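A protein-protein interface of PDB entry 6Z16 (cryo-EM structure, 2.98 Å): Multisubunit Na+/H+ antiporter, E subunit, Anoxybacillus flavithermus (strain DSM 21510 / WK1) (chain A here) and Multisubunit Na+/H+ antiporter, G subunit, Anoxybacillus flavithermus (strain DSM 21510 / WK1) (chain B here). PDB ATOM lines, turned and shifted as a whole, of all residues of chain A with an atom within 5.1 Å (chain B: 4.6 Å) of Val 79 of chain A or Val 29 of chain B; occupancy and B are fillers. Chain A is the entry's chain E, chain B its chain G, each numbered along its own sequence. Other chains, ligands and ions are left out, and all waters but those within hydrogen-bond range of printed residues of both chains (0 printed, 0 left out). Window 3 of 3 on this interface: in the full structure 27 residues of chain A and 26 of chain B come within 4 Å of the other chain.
The guanidinium group (NH2) of Arg 33 of chain B sits at hydrogen-bond distance from the side-chain hydroxyl (OG) of Ser 83 of chain A (3.1 Å).
The backbone carbonyl oxygen (O) of Lys 77 of chain A lies close to the side-chain amide oxygen (OE1) of Gln 81 of chain A (3.5 Å).
O of Gln 81 of chain A lies within hydrogen-bond range of OG of Ser 83 of chain A (3.5 Å).
Among the printed residues, merely in contact across the chains: Ala 76 of chain A with Leu 26 of chain B, Val 79 of chain A with Gly 30 of chain B, Val 79 of chain A with Leu 26 of chain B, Val 79 of chain A with Val 29 of chain B, Val 79 of chain A with Arg 33 of chain B and Gln 81 of chain A with Arg 33 of chain B.
Printed residues of chain B within 4 Å of Val 79 of chain A: Leu 26 (3.8 Å), Val 29 (3.8 Å), Gly 30 (3.8 Å) and Arg 33 (3.96 Å).
Val 29 of chain B touches one residue of chain A.
Printed residues of chain A within 4 Å of Gly 30 of chain B: Val 79 (3.8 Å).
Printed residues of chain B within 4 Å of Ser 83 of chain A: Arg 33.
Of the printed residues of chain B, Ala 76 of chain A touches Leu 26 (3.7 Å).
Leu 25 of chain B touches none of the printed residues of chain A.
Lys 77 of chain A touches none of the printed residues of chain B.
The nearest residue of chain B that does not touch Val 79 of chain A is Leu 34 of chain B (4.3 Å).
The nearest printed residue of chain A that does not touch Val 29 of chain B is Met 80 of chain A (6.2 Å).
The nearest printed residue of chain A that does not touch Arg 33 of chain B is Met 80 of chain A (5.9 Å).
Of the 8 printed residues of chain A, 4 touch a printed residue of chain B.
Printed residues of chain B that touch a printed residue of chain A: Leu 26, Val 29, Gly 30 and Arg 33.
Hydrophobic or aromatic side chains of chain B that line the printed part of chain A: Leu 26 and Val 29.
Along chain B the printed residues that touch a printed residue of chain A span positions 26 to 33.
Among the printed residues, 7 pairs touch across the chains.
Among the printed residues, no Asp or Glu carboxylate lies within 4 Å of a Lys or Arg side-chain nitrogen of the other chain.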
ATOM      1  N   VAL A  75       7.567  -5.755 -12.264  1.00  0.00           N
ATOM      2  CA  VAL A  75       6.648  -4.871 -11.547  1.00  0.00           C
ATOM      3  C   VAL A  75       6.984  -4.837 -10.056  1.00  0.00           C
ATOM      4  O   VAL A  75       6.877  -3.782  -9.414  1.00  0.00           O
ATOM      5  CB  VAL A  75       5.191  -5.302 -11.825  1.00  0.00           C
ATOM      6  CG1 VAL A  75       4.190  -4.543 -10.968  1.00  0.00           C
ATOM      7  CG2 VAL A  75       4.858  -5.067 -13.284  1.00  0.00           C
ATOM      8  N   ALA A  76       7.461  -5.960  -9.504  1.00  0.00           N
ATOM      9  CA  ALA A  76       7.897  -6.000  -8.112  1.00  0.00           C
ATOM     10  C   ALA A  76       9.082  -5.079  -7.860  1.00  0.00           C
ATOM     11  O   ALA A  76       9.131  -4.390  -6.835  1.00  0.00           O
ATOM     12  CB  ALA A  76       8.257  -7.432  -7.719  1.00  0.00           C
ATOM     13  N   LYS A  77      10.044  -5.045  -8.780  1.00  0.00           N
ATOM     14  CA  LYS A  77      11.166  -4.140  -8.558  1.00  0.00           C
ATOM     15  C   LYS A  77      10.873  -2.711  -8.998  1.00  0.00           C
ATOM     16  O   LYS A  77      11.676  -1.822  -8.704  1.00  0.00           O
ATOM     17  CB  LYS A  77      12.438  -4.638  -9.253  1.00  0.00           C
ATOM     18  CG  LYS A  77      12.463  -4.547 -10.766  1.00  0.00           C
ATOM     19  CD  LYS A  77      13.819  -5.010 -11.277  1.00  0.00           C
ATOM     20  CE  LYS A  77      13.949  -4.905 -12.787  1.00  0.00           C
ATOM     21  NZ  LYS A  77      13.130  -5.915 -13.508  1.00  0.00           N
ATOM     22  N   VAL A  78       9.769  -2.462  -9.704  1.00  0.00           N
ATOM     23  CA  VAL A  78       9.386  -1.078  -9.980  1.00  0.00           C
ATOM     24  C   VAL A  78       8.614  -0.472  -8.809  1.00  0.00           C
ATOM     25  O   VAL A  78       8.881   0.664  -8.401  1.00  0.00           O
ATOM     26  CB  VAL A  78       8.597  -0.998 -11.302  1.00  0.00           C
ATOM     27  CG1 VAL A  78       7.900   0.338 -11.451  1.00  0.00           C
ATOM     28  CG2 VAL A  78       9.543  -1.176 -12.475  1.00  0.00           C
ATOM     29  N   VAL A  79       7.678  -1.225  -8.224  1.00  0.00           N
ATOM     30  CA  VAL A  79       6.785  -0.659  -7.212  1.00  0.00           C
ATOM     31  C   VAL A  79       7.522  -0.425  -5.895  1.00  0.00           C
ATOM     32  O   VAL A  79       7.419   0.652  -5.297  1.00  0.00           O
ATOM     33  CB  VAL A  79       5.550  -1.560  -7.026  1.00  0.00           C
ATOM     34  CG1 VAL A  79       4.730  -1.113  -5.837  1.00  0.00           C
ATOM     35  CG2 VAL A  79       4.690  -1.517  -8.275  1.00  0.00           C
ATOM     36  N   MET A  80       8.294  -1.411  -5.432  1.00  0.00           N
ATOM     37  CA  MET A  80       9.053  -1.240  -4.196  1.00  0.00           C
ATOM     38  C   MET A  80      10.230  -0.283  -4.347  1.00  0.00           C
ATOM     39  O   MET A  80      10.780   0.158  -3.333  1.00  0.00           O
ATOM     40  CB  MET A  80       9.558  -2.589  -3.683  1.00  0.00           C
ATOM     41  CG  MET A  80       8.465  -3.536  -3.248  1.00  0.00           C
ATOM     42  SD  MET A  80       9.120  -5.013  -2.447  1.00  0.00           S
ATOM     43  CE  MET A  80       9.805  -5.903  -3.839  1.00  0.00           C
ATOM     44  N   GLN A  81      10.633   0.033  -5.574  1.00  0.00           N
ATOM     45  CA  GLN A  81      11.581   1.108  -5.822  1.00  0.00           C
ATOM     46  C   GLN A  81      10.935   2.443  -5.464  1.00  0.00           C
ATOM     47  O   GLN A  81       9.708   2.572  -5.442  1.00  0.00           O
ATOM     48  CB  GLN A  81      12.004   1.095  -7.296  1.00  0.00           C
ATOM     49  CG  GLN A  81      13.190   1.969  -7.702  1.00  0.00           C
ATOM     50  CD  GLN A  81      13.509   1.871  -9.186  1.00  0.00           C
ATOM     51  OE1 GLN A  81      12.782   1.233  -9.947  1.00  0.00           O
ATOM     52  NE2 GLN A  81      14.608   2.486  -9.598  1.00  0.00           N
ATOM     53  N   SER A  83       9.445   5.616  -6.351  1.00  0.00           N
ATOM     54  CA  SER A  83       8.585   5.649  -7.533  1.00  0.00           C
ATOM     55  C   SER A  83       8.779   6.886  -8.417  1.00  0.00           C
ATOM     56  O   SER A  83       7.914   7.174  -9.252  1.00  0.00           O
ATOM     57  CB  SER A  83       7.118   5.543  -7.108  1.00  0.00           C
ATOM     58  OG  SER A  83       6.863   4.305  -6.469  1.00  0.00           O
ATOM     59  N   LEU B  25      -1.099  -7.961  -2.556  1.00  0.00           N
ATOM     60  CA  LEU B  25      -0.837  -6.731  -1.804  1.00  0.00           C
ATOM     61  C   LEU B  25       0.140  -5.819  -2.534  1.00  0.00           C
ATOM     62  O   LEU B  25       0.034  -4.589  -2.445  1.00  0.00           O
ATOM     63  CB  LEU B  25      -0.298  -7.062  -0.419  1.00  0.00           C
ATOM     64  CG  LEU B  25      -0.049  -5.931   0.580  1.00  0.00           C
ATOM     65  CD1 LEU B  25      -1.337  -5.203   0.907  1.00  0.00           C
ATOM     66  CD2 LEU B  25       0.580  -6.487   1.841  1.00  0.00           C
ATOM     67  N   LEU B  26       1.088  -6.407  -3.260  1.00  0.00           N
ATOM     68  CA  LEU B  26       1.975  -5.629  -4.115  1.00  0.00           C
ATOM     69  C   LEU B  26       1.210  -4.962  -5.250  1.00  0.00           C
ATOM     70  O   LEU B  26       1.505  -3.817  -5.614  1.00  0.00           O
ATOM     71  CB  LEU B  26       3.073  -6.529  -4.661  1.00  0.00           C
ATOM     72  CG  LEU B  26       4.075  -5.915  -5.626  1.00  0.00           C
ATOM     73  CD1 LEU B  26       4.877  -4.807  -4.969  1.00  0.00           C
ATOM     74  CD2 LEU B  26       4.960  -7.023  -6.104  1.00  0.00           C
ATOM     75  N   SER B  27       0.214  -5.660  -5.806  1.00  0.00           N
ATOM     76  CA  SER B  27      -0.673  -5.038  -6.789  1.00  0.00           C
ATOM     77  C   SER B  27      -1.436  -3.862  -6.190  1.00  0.00           C
ATOM     78  O   SER B  27      -1.643  -2.842  -6.854  1.00  0.00           O
ATOM     79  CB  SER B  27      -1.652  -6.069  -7.342  1.00  0.00           C
ATOM     80  OG  SER B  27      -2.568  -5.463  -8.232  1.00  0.00           O
ATOM     81  N   ALA B  28      -1.832  -3.979  -4.922  1.00  0.00           N
ATOM     82  CA  ALA B  28      -2.578  -2.900  -4.274  1.00  0.00           C
ATOM     83  C   ALA B  28      -1.704  -1.679  -4.000  1.00  0.00           C
ATOM     84  O   ALA B  28      -2.128  -0.538  -4.232  1.00  0.00           O
ATOM     85  CB  ALA B  28      -3.195  -3.403  -2.980  1.00  0.00           C
ATOM     86  N   VAL B  29      -0.482  -1.892  -3.501  1.00  0.00           N
ATOM     87  CA  VAL B  29       0.393  -0.748  -3.255  1.00  0.00           C
ATOM     88  C   VAL B  29       0.895  -0.144  -4.562  1.00  0.00           C
ATOM     89  O   VAL B  29       1.192   1.055  -4.607  1.00  0.00           O
ATOM     90  CB  VAL B  29       1.562  -1.113  -2.314  1.00  0.00           C
ATOM     91  CG1 VAL B  29       1.035  -1.602  -0.978  1.00  0.00           C
ATOM     92  CG2 VAL B  29       2.484  -2.132  -2.927  1.00  0.00           C
ATOM     93  N   GLY B  30       0.944  -0.925  -5.646  1.00  0.00           N
ATOM     94  CA  GLY B  30       1.187  -0.339  -6.951  1.00  0.00           C
ATOM     95  C   GLY B  30      -0.005   0.425  -7.489  1.00  0.00           C
ATOM     96  O   GLY B  30       0.158   1.371  -8.261  1.00  0.00           O
ATOM     97  N   ALA B  31      -1.217   0.020  -7.104  1.00  0.00           N
ATOM     98  CA  ALA B  31      -2.400   0.794  -7.459  1.00  0.00           C
ATOM     99  C   ALA B  31      -2.414   2.135  -6.739  1.00  0.00           C
ATOM    100  O   ALA B  31      -2.831   3.150  -7.308  1.00  0.00           O
ATOM    101  CB  ALA B  31      -3.664   0.005  -7.125  1.00  0.00           C
ATOM    102  N   ILE B  32      -1.956   2.152  -5.487  1.00  0.00           N
ATOM    103  CA  ILE B  32      -1.917   3.397  -4.720  1.00  0.00           C
ATOM    104  C   ILE B  32      -0.811   4.319  -5.228  1.00  0.00           C
ATOM    105  O   ILE B  32      -1.045   5.500  -5.507  1.00  0.00           O
ATOM    106  CB  ILE B  32      -1.755   3.097  -3.220  1.00  0.00           C
ATOM    107  CG1 ILE B  32      -3.006   2.411  -2.684  1.00  0.00           C
ATOM    108  CG2 ILE B  32      -1.467   4.362  -2.444  1.00  0.00           C
ATOM    109  CD1 ILE B  32      -2.848   1.865  -1.294  1.00  0.00           C
ATOM    110  N   ARG B  33       0.405   3.791  -5.386  1.00  0.00           N
ATOM    111  CA  ARG B  33       1.586   4.638  -5.528  1.00  0.00           C
ATOM    112  C   ARG B  33       1.862   5.123  -6.947  1.00  0.00           C
ATOM    113  O   ARG B  33       2.588   6.109  -7.109  1.00  0.00           O
ATOM    114  CB  ARG B  33       2.808   3.893  -5.005  1.00  0.00           C
ATOM    115  CG  ARG B  33       2.826   3.774  -3.500  1.00  0.00           C
ATOM    116  CD  ARG B  33       3.986   2.933  -3.028  1.00  0.00           C
ATOM    117  NE  ARG B  33       5.263   3.452  -3.507  1.00  0.00           N
ATOM    118  CZ  ARG B  33       5.946   4.435  -2.930  1.00  0.00           C
ATOM    119  NH1 ARG B  33       5.474   5.033  -1.847  1.00  0.00           N
ATOM    120  NH2 ARG B  33       7.103   4.822  -3.443  1.00  0.00           N
ATOM    121  N   LEU B  34       1.327   4.482  -7.961  1.00  0.00           N
ATOM    122  CA  LEU B  34       1.740   4.848  -9.313  1.00  0.00           C
ATOM    123  C   LEU B  34       0.891   6.006  -9.844  1.00  0.00           C
ATOM    124  O   LEU B  34      -0.303   6.080  -9.556  1.00  0.00           O
ATOM    125  CB  LEU B  34       1.645   3.635 -10.231  1.00  0.00           C
ATOM    126  CG  LEU B  34       2.720   2.595  -9.905  1.00  0.00           C
ATOM    127  CD1 LEU B  34       2.520   1.331 -10.699  1.00  0.00           C
ATOM    128  CD2 LEU B  34       4.101   3.166 -10.157  1.00  0.00           C
